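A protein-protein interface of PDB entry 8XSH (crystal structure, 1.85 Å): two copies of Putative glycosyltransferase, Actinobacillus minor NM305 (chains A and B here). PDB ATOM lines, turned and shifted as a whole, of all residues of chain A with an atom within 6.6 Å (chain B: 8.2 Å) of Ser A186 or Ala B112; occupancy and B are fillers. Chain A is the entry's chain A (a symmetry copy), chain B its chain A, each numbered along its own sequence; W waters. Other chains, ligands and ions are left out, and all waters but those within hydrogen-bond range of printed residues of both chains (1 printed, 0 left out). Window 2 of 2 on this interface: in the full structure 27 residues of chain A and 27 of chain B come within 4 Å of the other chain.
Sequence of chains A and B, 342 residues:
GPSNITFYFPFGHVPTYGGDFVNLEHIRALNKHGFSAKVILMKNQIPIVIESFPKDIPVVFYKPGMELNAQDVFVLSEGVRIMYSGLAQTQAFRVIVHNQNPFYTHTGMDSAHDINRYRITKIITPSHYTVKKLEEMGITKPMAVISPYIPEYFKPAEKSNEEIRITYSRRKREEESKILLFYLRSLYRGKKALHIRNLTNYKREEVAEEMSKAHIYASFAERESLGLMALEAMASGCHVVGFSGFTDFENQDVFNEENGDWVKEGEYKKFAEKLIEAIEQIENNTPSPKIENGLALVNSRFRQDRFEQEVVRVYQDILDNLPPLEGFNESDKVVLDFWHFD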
ATOM      1  N   LEU A 181      29.036 -12.081  -4.304  1.00  0.00           N
ATOM      2  CA  LEU A 181      29.933 -13.220  -4.201  1.00  0.00           C
ATOM      3  C   LEU A 181      29.554 -14.041  -2.966  1.00  0.00           C
ATOM      4  O   LEU A 181      29.634 -15.250  -3.026  1.00  0.00           O
ATOM      5  CB  LEU A 181      31.385 -12.747  -4.214  1.00  0.00           C
ATOM      6  CG  LEU A 181      31.863 -12.234  -5.581  1.00  0.00           C
ATOM      7  CD1 LEU A 181      33.255 -11.609  -5.507  1.00  0.00           C
ATOM      8  CD2 LEU A 181      31.858 -13.319  -6.645  1.00  0.00           C
ATOM      9  N   PHE A 182      29.035 -13.379  -1.907  1.00  0.00           N
ATOM     10  CA  PHE A 182      28.503 -14.077  -0.749  1.00  0.00           C
ATOM     11  C   PHE A 182      27.298 -14.945  -1.099  1.00  0.00           C
ATOM     12  O   PHE A 182      27.231 -16.116  -0.684  1.00  0.00           O
ATOM     13  CB  PHE A 182      28.179 -13.102   0.383  1.00  0.00           C
ATOM     14  CG  PHE A 182      27.640 -13.790   1.617  1.00  0.00           C
ATOM     15  CD1 PHE A 182      28.504 -14.293   2.589  1.00  0.00           C
ATOM     16  CD2 PHE A 182      26.270 -13.906   1.827  1.00  0.00           C
ATOM     17  CE1 PHE A 182      28.018 -14.868   3.747  1.00  0.00           C
ATOM     18  CE2 PHE A 182      25.785 -14.527   2.968  1.00  0.00           C
ATOM     19  CZ  PHE A 182      26.667 -15.001   3.924  1.00  0.00           C
ATOM     20  N   TYR A 183      26.364 -14.412  -1.895  1.00  0.00           N
ATOM     21  CA  TYR A 183      25.274 -15.231  -2.363  1.00  0.00           C
ATOM     22  C   TYR A 183      25.793 -16.403  -3.203  1.00  0.00           C
ATOM     23  O   TYR A 183      25.255 -17.487  -3.106  1.00  0.00           O
ATOM     24  CB  TYR A 183      24.289 -14.457  -3.229  1.00  0.00           C
ATOM     25  CG  TYR A 183      23.239 -13.665  -2.497  1.00  0.00           C
ATOM     26  CD1 TYR A 183      23.524 -12.430  -1.915  1.00  0.00           C
ATOM     27  CD2 TYR A 183      21.931 -14.123  -2.426  1.00  0.00           C
ATOM     28  CE1 TYR A 183      22.529 -11.677  -1.305  1.00  0.00           C
ATOM     29  CE2 TYR A 183      20.920 -13.368  -1.825  1.00  0.00           C
ATOM     30  CZ  TYR A 183      21.229 -12.148  -1.253  1.00  0.00           C
ATOM     31  OH  TYR A 183      20.198 -11.460  -0.644  1.00  0.00           O
ATOM     32  N   LEU A 184      26.789 -16.171  -4.053  1.00  0.00           N
ATOM     33  CA  LEU A 184      27.282 -17.212  -4.950  1.00  0.00           C
ATOM     34  C   LEU A 184      27.912 -18.326  -4.123  1.00  0.00           C
ATOM     35  O   LEU A 184      27.635 -19.504  -4.360  1.00  0.00           O
ATOM     36  CB  LEU A 184      28.254 -16.602  -5.964  1.00  0.00           C
ATOM     37  CG  LEU A 184      28.906 -17.585  -6.934  1.00  0.00           C
ATOM     38  CD1 LEU A 184      27.865 -18.265  -7.791  1.00  0.00           C
ATOM     39  CD2 LEU A 184      29.961 -16.902  -7.812  1.00  0.00           C
ATOM     40  N   ARG A 185      28.743 -17.958  -3.147  1.00  0.00           N
ATOM     41  CA  ARG A 185      29.349 -18.962  -2.280  1.00  0.00           C
ATOM     42  C   ARG A 185      28.272 -19.733  -1.506  1.00  0.00           C
ATOM     43  O   ARG A 185      28.435 -20.929  -1.242  1.00  0.00           O
ATOM     44  CB  ARG A 185      30.335 -18.316  -1.308  1.00  0.00           C
ATOM     45  CG  ARG A 185      31.620 -17.771  -1.916  1.00  0.00           C
ATOM     46  CD  ARG A 185      32.617 -17.403  -0.816  1.00  0.00           C
ATOM     47  NE  ARG A 185      32.201 -16.321   0.075  1.00  0.00           N
ATOM     48  CZ  ARG A 185      32.245 -15.025  -0.195  1.00  0.00           C
ATOM     49  NH1 ARG A 185      32.694 -14.612  -1.357  1.00  0.00           N
ATOM     50  NH2 ARG A 185      31.891 -14.139   0.718  1.00  0.00           N
ATOM     51  N   SER A 186      27.175 -19.060  -1.144  1.00  0.00           N
ATOM     52  CA  SER A 186      26.104 -19.631  -0.345  1.00  0.00           C
ATOM     53  C   SER A 186      25.230 -20.584  -1.160  1.00  0.00           C
ATOM     54  O   SER A 186      24.651 -21.522  -0.600  1.00  0.00           O
ATOM     55  CB  SER A 186      25.234 -18.533   0.271  1.00  0.00           C
ATOM     56  OG  SER A 186      25.943 -17.795   1.257  1.00  0.00           O
ATOM     57  N   LEU A 187      25.086 -20.310  -2.462  1.00  0.00           N
ATOM     58  CA  LEU A 187      24.126 -21.026  -3.299  1.00  0.00           C
ATOM     59  C   LEU A 187      24.805 -22.048  -4.215  1.00  0.00           C
ATOM     60  O   LEU A 187      24.166 -23.020  -4.598  1.00  0.00           O
ATOM     61  CB  LEU A 187      23.305 -20.011  -4.107  1.00  0.00           C
ATOM     62  CG  LEU A 187      22.313 -19.179  -3.288  1.00  0.00           C
ATOM     63  CD1 LEU A 187      21.636 -18.134  -4.170  1.00  0.00           C
ATOM     64  CD2 LEU A 187      21.273 -20.072  -2.578  1.00  0.00           C
ATOM     65  N   TYR A 188      26.093 -21.890  -4.549  1.00  0.00           N
ATOM     66  CA  TYR A 188      26.736 -22.805  -5.497  1.00  0.00           C
ATOM     67  C   TYR A 188      27.104 -24.135  -4.838  1.00  0.00           C
ATOM     68  O   TYR A 188      27.900 -24.163  -3.919  1.00  0.00           O
ATOM     69  CB  TYR A 188      27.998 -22.165  -6.094  1.00  0.00           C
ATOM     70  CG  TYR A 188      28.796 -23.060  -7.014  1.00  0.00           C
ATOM     71  CD1 TYR A 188      28.239 -23.578  -8.168  1.00  0.00           C
ATOM     72  CD2 TYR A 188      30.100 -23.428  -6.703  1.00  0.00           C
ATOM     73  CE1 TYR A 188      28.966 -24.390  -9.019  1.00  0.00           C
ATOM     74  CE2 TYR A 188      30.836 -24.256  -7.529  1.00  0.00           C
ATOM     75  CZ  TYR A 188      30.270 -24.724  -8.703  1.00  0.00           C
ATOM     76  OH  TYR A 188      30.973 -25.559  -9.521  1.00  0.00           O
ATOM     77  N   ARG A 189      26.563 -25.246  -5.346  1.00  0.00           N
ATOM     78  CA  ARG A 189      26.843 -26.559  -4.786  1.00  0.00           C
ATOM     79  C   ARG A 189      27.556 -27.485  -5.773  1.00  0.00           C
ATOM     80  O   ARG A 189      27.659 -28.676  -5.494  1.00  0.00           O
ATOM     81  CB  ARG A 189      25.531 -27.190  -4.317  1.00  0.00           C
ATOM     82  CG  ARG A 189      25.079 -26.709  -2.949  1.00  0.00           C
ATOM     83  CD  ARG A 189      23.575 -26.769  -2.899  1.00  0.00           C
ATOM     84  NE  ARG A 189      23.087 -26.887  -1.537  1.00  0.00           N
ATOM     85  CZ  ARG A 189      22.474 -25.923  -0.862  1.00  0.00           C
ATOM     86  NH1 ARG A 189      22.523 -24.672  -1.298  1.00  0.00           N
ATOM     87  NH2 ARG A 189      21.865 -26.211   0.276  1.00  0.00           N
ATOM     88  N   THR B 105      26.773  -9.462   6.043  1.00  0.00           N
ATOM     89  CA  THR B 105      26.964 -10.775   6.634  1.00  0.00           C
ATOM     90  C   THR B 105      28.289 -11.367   6.143  1.00  0.00           C
ATOM     91  O   THR B 105      28.936 -12.119   6.874  1.00  0.00           O
ATOM     92  CB  THR B 105      25.776 -11.704   6.347  1.00  0.00           C
ATOM     93  OG1 THR B 105      24.597 -11.068   6.822  1.00  0.00           O
ATOM     94  CG2 THR B 105      25.938 -13.077   6.976  1.00  0.00           C
ATOM     95  N   HIS B 106      28.726 -10.964   4.948  1.00  0.00           N
ATOM     96  CA  HIS B 106      29.965 -11.459   4.352  1.00  0.00           C
ATOM     97  C   HIS B 106      31.217 -11.020   5.110  1.00  0.00           C
ATOM     98  O   HIS B 106      32.302 -11.567   4.873  1.00  0.00           O
ATOM     99  CB  HIS B 106      30.046 -11.058   2.875  1.00  0.00           C
ATOM    100  CG  HIS B 106      30.154  -9.608   2.682  1.00  0.00           C
ATOM    101  ND1 HIS B 106      31.295  -8.885   2.966  1.00  0.00           N
ATOM    102  CD2 HIS B 106      29.212  -8.727   2.313  1.00  0.00           C
ATOM    103  CE1 HIS B 106      31.044  -7.607   2.733  1.00  0.00           C
ATOM    104  NE2 HIS B 106      29.789  -7.493   2.344  1.00  0.00           N
ATOM    105  N   MET B 109      31.363 -14.237   8.113  1.00  0.00           N
ATOM    106  CA  MET B 109      31.280 -15.661   7.852  1.00  0.00           C
ATOM    107  C   MET B 109      31.369 -15.830   6.349  1.00  0.00           C
ATOM    108  O   MET B 109      30.918 -14.953   5.629  1.00  0.00           O
ATOM    109  CB  MET B 109      29.940 -16.228   8.335  1.00  0.00           C
ATOM    110  CG  MET B 109      29.846 -16.386   9.826  1.00  0.00           C
ATOM    111  SD  MET B 109      31.039 -17.576  10.524  1.00  0.00           S
ATOM    112  CE  MET B 109      29.913 -18.878  11.018  1.00  0.00           C
ATOM    113  N   ASP B 110      31.911 -16.960   5.892  1.00  0.00           N
ATOM    114  CA  ASP B 110      32.226 -17.139   4.479  1.00  0.00           C
ATOM    115  C   ASP B 110      30.961 -17.272   3.620  1.00  0.00           C
ATOM    116  O   ASP B 110      30.920 -16.791   2.472  1.00  0.00           O
ATOM    117  CB  ASP B 110      33.156 -18.346   4.261  1.00  0.00           C
ATOM    118  CG  ASP B 110      33.587 -18.440   2.807  1.00  0.00           C
ATOM    119  OD1 ASP B 110      34.251 -17.464   2.331  1.00  0.00           O
ATOM    120  OD2 ASP B 110      33.192 -19.433   2.139  1.00  0.00           O
ATOM    121  N   SER B 111      29.945 -17.963   4.172  1.00  0.00           N
ATOM    122  CA  SER B 111      28.757 -18.328   3.415  1.00  0.00           C
ATOM    123  C   SER B 111      27.641 -18.697   4.383  1.00  0.00           C
ATOM    124  O   SER B 111      27.876 -18.833   5.583  1.00  0.00           O
ATOM    125  CB  SER B 111      29.044 -19.500   2.485  1.00  0.00           C
ATOM    126  OG  SER B 111      29.009 -20.719   3.217  1.00  0.00           O
ATOM    127  N   ALA B 112      26.435 -18.901   3.845  1.00  0.00           N
ATOM    128  CA  ALA B 112      25.324 -19.356   4.664  1.00  0.00           C
ATOM    129  C   ALA B 112      25.661 -20.713   5.272  1.00  0.00           C
ATOM    130  O   ALA B 112      25.192 -21.018   6.373  1.00  0.00           O
ATOM    131  CB  ALA B 112      24.057 -19.431   3.846  1.00  0.00           C
ATOM    132  N   HIS B 113      26.410 -21.534   4.517  1.00  0.00           N
ATOM    133  CA  HIS B 113      26.744 -22.893   4.946  1.00  0.00           C
ATOM    134  C   HIS B 113      27.487 -22.856   6.273  1.00  0.00           C
ATOM    135  O   HIS B 113      27.210 -23.650   7.159  1.00  0.00           O
ATOM    136  CB  HIS B 113      27.581 -23.656   3.909  1.00  0.00           C
ATOM    137  CG  HIS B 113      26.931 -23.822   2.584  1.00  0.00           C
ATOM    138  ND1 HIS B 113      27.530 -23.436   1.393  1.00  0.00           N
ATOM    139  CD2 HIS B 113      25.701 -24.277   2.262  1.00  0.00           C
ATOM    140  CE1 HIS B 113      26.700 -23.682   0.383  1.00  0.00           C
ATOM    141  NE2 HIS B 113      25.574 -24.186   0.890  1.00  0.00           N
ATOM    142  N   ASP B 114      28.414 -21.909   6.401  1.00  0.00           N
ATOM    143  CA  ASP B 114      29.234 -21.767   7.591  1.00  0.00           C
ATOM    144  C   ASP B 114      28.405 -21.293   8.785  1.00  0.00           C
ATOM    145  O   ASP B 114      28.580 -21.770   9.910  1.00  0.00           O
ATOM    146  CB  ASP B 114      30.374 -20.794   7.323  1.00  0.00           C
ATOM    147  CG  ASP B 114      31.294 -21.303   6.233  1.00  0.00           C
ATOM    148  OD1 ASP B 114      32.069 -22.190   6.523  1.00  0.00           O
ATOM    149  OD2 ASP B 114      31.168 -20.831   5.081  1.00  0.00           O
ATOM    150  N   ILE B 115      27.473 -20.388   8.520  1.00  0.00           N
ATOM    151  CA  ILE B 115      26.540 -19.943   9.542  1.00  0.00           C
ATOM    152  C   ILE B 115      25.675 -21.121   9.974  1.00  0.00           C
ATOM    153  O   ILE B 115      25.457 -21.312  11.168  1.00  0.00           O
ATOM    154  CB  ILE B 115      25.710 -18.754   9.037  1.00  0.00           C
ATOM    155  CG1 ILE B 115      26.590 -17.518   8.858  1.00  0.00           C
ATOM    156  CG2 ILE B 115      24.526 -18.446   9.934  1.00  0.00           C
ATOM    157  CD1 ILE B 115      25.914 -16.380   8.060  1.00  0.00           C
ATOM    158  N   ASN B 116      25.204 -21.912   9.007  1.00  0.00           N
ATOM    159  CA  ASN B 116      24.254 -22.966   9.315  1.00  0.00           C
ATOM    160  C   ASN B 116      24.918 -24.086  10.115  1.00  0.00           C
ATOM    161  O   ASN B 116      24.284 -24.768  10.917  1.00  0.00           O
ATOM    162  CB  ASN B 116      23.622 -23.556   8.064  1.00  0.00           C
ATOM    163  CG  ASN B 116      22.622 -22.627   7.423  1.00  0.00           C
ATOM    164  OD1 ASN B 116      22.108 -21.700   8.063  1.00  0.00           O
ATOM    165  ND2 ASN B 116      22.386 -22.863   6.145  1.00  0.00           N
ATOM    166  N   ARG B 117      26.225 -24.249   9.931  1.00  0.00           N
ATOM    167  CA  ARG B 117      26.937 -25.308  10.632  1.00  0.00           C
ATOM    168  C   ARG B 117      27.449 -24.836  11.994  1.00  0.00           C
ATOM    169  O   ARG B 117      27.792 -25.661  12.829  1.00  0.00           O
ATOM    170  CB  ARG B 117      28.065 -25.839   9.747  1.00  0.00           C
ATOM    171  CG  ARG B 117      27.552 -26.668   8.577  1.00  0.00           C
ATOM    172  CD  ARG B 117      28.657 -27.364   7.799  1.00  0.00           C
ATOM    173  NE  ARG B 117      28.866 -26.717   6.504  1.00  0.00           N
ATOM    174  CZ  ARG B 117      29.883 -25.909   6.249  1.00  0.00           C
ATOM    175  NH1 ARG B 117      30.747 -25.646   7.218  1.00  0.00           N
ATOM    176  NH2 ARG B 117      30.003 -25.343   5.058  1.00  0.00           N
ATOM    177  N   TYR B 118      27.491 -23.522  12.235  1.00  0.00           N
ATOM    178  CA  TYR B 118      27.980 -22.990  13.501  1.00  0.00           C
ATOM    179  C   TYR B 118      26.923 -23.188  14.593  1.00  0.00           C
ATOM    180  O   TYR B 118      25.720 -23.145  14.330  1.00  0.00           O
ATOM    181  CB  TYR B 118      28.328 -21.503  13.349  1.00  0.00           C
ATOM    182  CG  TYR B 118      29.346 -20.968  14.333  1.00  0.00           C
ATOM    183  CD1 TYR B 118      30.690 -20.938  14.010  1.00  0.00           C
ATOM    184  CD2 TYR B 118      28.993 -20.529  15.592  1.00  0.00           C
ATOM    185  CE1 TYR B 118      31.653 -20.489  14.893  1.00  0.00           C
ATOM    186  CE2 TYR B 118      29.941 -20.064  16.497  1.00  0.00           C
ATOM    187  CZ  TYR B 118      31.278 -20.031  16.142  1.00  0.00           C
ATOM    188  OH  TYR B 118      32.237 -19.593  17.021  1.00  0.00           O
ATOM    189  N   ILE B 120      25.166 -21.473  16.463  1.00  0.00           N
ATOM    190  CA  ILE B 120      24.383 -20.283  16.728  1.00  0.00           C
ATOM    191  C   ILE B 120      23.040 -20.730  17.286  1.00  0.00           C
ATOM    192  O   ILE B 120      22.366 -21.519  16.653  1.00  0.00           O
ATOM    193  CB  ILE B 120      24.207 -19.429  15.458  1.00  0.00           C
ATOM    194  CG1 ILE B 120      25.560 -18.910  14.951  1.00  0.00           C
ATOM    195  CG2 ILE B 120      23.205 -18.285  15.670  1.00  0.00           C
ATOM    196  CD1 ILE B 120      25.566 -18.402  13.518  1.00  0.00           C
ATOM    197  N   LEU B 134      18.014 -12.769   5.135  1.00  0.00           N
ATOM    198  CA  LEU B 134      18.966 -13.795   5.533  1.00  0.00           C
ATOM    199  C   LEU B 134      18.513 -15.165   5.051  1.00  0.00           C
ATOM    200  O   LEU B 134      19.346 -15.957   4.644  1.00  0.00           O
ATOM    201  CB  LEU B 134      19.131 -13.806   7.053  1.00  0.00           C
ATOM    202  CG  LEU B 134      19.717 -12.530   7.645  1.00  0.00           C
ATOM    203  CD1 LEU B 134      19.827 -12.650   9.157  1.00  0.00           C
ATOM    204  CD2 LEU B 134      21.062 -12.200   7.019  1.00  0.00           C
ATOM    205  N   GLU B 135      17.207 -15.426   5.086  1.00  0.00           N
ATOM    206  CA  GLU B 135      16.648 -16.685   4.620  1.00  0.00           C
ATOM    207  C   GLU B 135      16.812 -16.811   3.098  1.00  0.00           C
ATOM    208  O   GLU B 135      17.117 -17.898   2.627  1.00  0.00           O
ATOM    209  CB  GLU B 135      15.188 -16.824   5.063  1.00  0.00           C
ATOM    210  CG  GLU B 135      15.027 -17.136   6.544  1.00  0.00           C
ATOM    211  CD  GLU B 135      13.590 -17.202   7.055  1.00  0.00           C
ATOM    212  OE1 GLU B 135      12.680 -16.830   6.315  1.00  0.00           O
ATOM    213  OE2 GLU B 135      13.386 -17.607   8.214  1.00  0.00           O
ATOM    214  N   GLU B 136      16.707 -15.699   2.353  1.00  0.00           N
ATOM    215  CA  GLU B 136      16.971 -15.667   0.914  1.00  0.00           C
ATOM    216  C   GLU B 136      18.405 -16.110   0.612  1.00  0.00           C
ATOM    217  O   GLU B 136      18.673 -16.757  -0.409  1.00  0.00           O
ATOM    218  CB  GLU B 136      16.730 -14.242   0.390  1.00  0.00           C
ATOM    219  CG  GLU B 136      16.926 -14.048  -1.102  1.00  0.00           C
ATOM    220  CD  GLU B 136      16.710 -12.627  -1.597  1.00  0.00           C
ATOM    221  OE1 GLU B 136      17.643 -11.747  -1.473  1.00  0.00           O
ATOM    222  OE2 GLU B 136      15.602 -12.396  -2.099  1.00  0.00           O
ATOM    223  N   MET B 137      19.318 -15.712   1.504  1.00  0.00           N
ATOM    224  CA  MET B 137      20.728 -15.995   1.374  1.00  0.00           C
ATOM    225  C   MET B 137      21.042 -17.449   1.697  1.00  0.00           C
ATOM    226  O   MET B 137      22.172 -17.848   1.458  1.00  0.00           O
ATOM    227  CB  MET B 137      21.572 -15.123   2.303  1.00  0.00           C
ATOM    228  CG  MET B 137      21.789 -13.720   1.796  1.00  0.00           C
ATOM    229  SD  MET B 137      22.357 -12.638   3.142  1.00  0.00           S
ATOM    230  CE  MET B 137      22.182 -11.031   2.369  1.00  0.00           C
ATOM    231  N   GLY B 138      20.088 -18.217   2.242  1.00  0.00           N
ATOM    232  CA  GLY B 138      20.313 -19.627   2.514  1.00  0.00           C
ATOM    233  C   GLY B 138      20.532 -19.932   3.995  1.00  0.00           C
ATOM    234  O   GLY B 138      20.811 -21.081   4.349  1.00  0.00           O
ATOM    235  N   ILE B 139      20.317 -18.945   4.879  1.00  0.00           N
ATOM    236  CA  ILE B 139      20.510 -19.176   6.306  1.00  0.00           C
ATOM    237  C   ILE B 139      19.244 -19.793   6.883  1.00  0.00           C
ATOM    238  O   ILE B 139      18.159 -19.287   6.610  1.00  0.00           O
ATOM    239  CB  ILE B 139      20.868 -17.872   7.038  1.00  0.00           C
ATOM    240  CG1 ILE B 139      22.207 -17.317   6.540  1.00  0.00           C
ATOM    241  CG2 ILE B 139      20.846 -18.128   8.532  1.00  0.00           C
ATOM    242  CD1 ILE B 139      22.458 -15.877   6.872  1.00  0.00           C
ATOM    243  N   THR B 140      19.400 -20.868   7.675  1.00  0.00           N
ATOM    244  CA  THR B 140      18.257 -21.614   8.200  1.00  0.00           C
ATOM    245  C   THR B 140      18.171 -21.585   9.726  1.00  0.00           C
ATOM    246  O   THR B 140      17.275 -22.198  10.280  1.00  0.00           O
ATOM    247  CB  THR B 140      18.261 -23.063   7.710  1.00  0.00           C
ATOM    248  OG1 THR B 140      19.498 -23.651   8.103  1.00  0.00           O
ATOM    249  CG2 THR B 140      18.130 -23.155   6.207  1.00  0.00           C
ATOM    250  N   LYS B 141      19.064 -20.856  10.393  1.00  0.00           N
ATOM    251  CA  LYS B 141      19.044 -20.695  11.838  1.00  0.00           C
ATOM    252  C   LYS B 141      17.770 -19.987  12.303  1.00  0.00           C
ATOM    253  O   LYS B 141      17.223 -19.152  11.600  1.00  0.00           O
ATOM    254  CB  LYS B 141      20.280 -19.913  12.281  1.00  0.00           C
ATOM    255  CG  LYS B 141      21.573 -20.705  12.212  1.00  0.00           C
ATOM    256  CD  LYS B 141      21.652 -21.774  13.295  1.00  0.00           C
ATOM    257  CE  LYS B 141      22.872 -22.663  13.142  1.00  0.00           C
ATOM    258  NZ  LYS B 141      23.067 -23.578  14.289  1.00  0.00           N
HETATM  259  O   HOH W   1      32.435 -13.656   3.534  1.00  0.00           O
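OG of Ser A186 lies within hydrogen-bond range of N of Ala B112. A ring nitrogen (NE2) of His B113 lies close to the backbone carbonyl oxygen of Ser A186, at 3.2 Å. The side-chain carboxylate (OD1) of Asp B110 is in salt-bridge range of the guanidinium group (NE) of Arg A185 (3.3 Å). OE1 of Glu B136 lies within hydrogen-bond range of OH of Tyr A183 (2.7 Å).
O of Ala B112 sits close to ND2 of Asn B116 (3.4 Å). OD2 of Asp B114 sits at hydrogen-bond distance from OG of Ser B111 (2.9 Å). OG of Ser B111 sits at hydrogen-bond distance from N of His B113, at 3.0 Å. O of Phe A182 is in hydrogen-bond range of OG of Ser A186, 2.9 Å away.
Phe A182 touches Thr B105 (CZ to CG2, 3.7 Å). CD1 of Phe A182 touches CB of His B106, 3.6 Å away. Phe A182 touches Met B109. Asp B110 touches Phe A182. Phe A182 touches Ala B112. Met B137 touches Phe A182 (SD to CE2, 3.9 Å). Tyr A183 touches Met B137. CA of Ser B111 touches OG of Ser A186, 3.6 Å away. Ser A186 touches Met B137. Arg A189 touches His B113 (NH1 to NE2, 3.8 Å).
Ser A186 touches just these residues of chain B: Ser B111, Ala B112, His B113 and Met B137. Printed residues of chain A within 4 Å of Thr B105: Phe A182. Of the printed residues of chain A, Asp B110 touches Phe A182 (3.5 Å) and Arg A185 (2.8 Å). Printed residues of chain A within 4 Å of Glu B136: Tyr A183 (2.7 Å). Ile B115 touches none of the printed residues of chain A. Lys B141 touches none of the printed residues of chain A. The nearest printed residue of chain A that does not touch Thr B105 is Arg A185 (7.1 Å).
Of the 9 printed residues of chain A, 5 touch a printed residue of chain B. Hydrophobic or aromatic side chains of chain A that line the printed part of chain B: Phe A182 and Tyr A183. Among the printed residues, 16 pairs touch across the chains. Among the printed residues, Asp or Glu carboxylates within 4 Å of a Lys or Arg side-chain nitrogen of the other chain: Arg A185 with Asp B110 (3.3 Å).
No position is printed for both chains. Of the 16 pairs that touch across the chains among the printed residues, none has its exchanged pair printed and touching as well.
Water W1 lies within hydrogen-bond range of O of His B106, O of Met B109 and NH2 of Arg A185.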
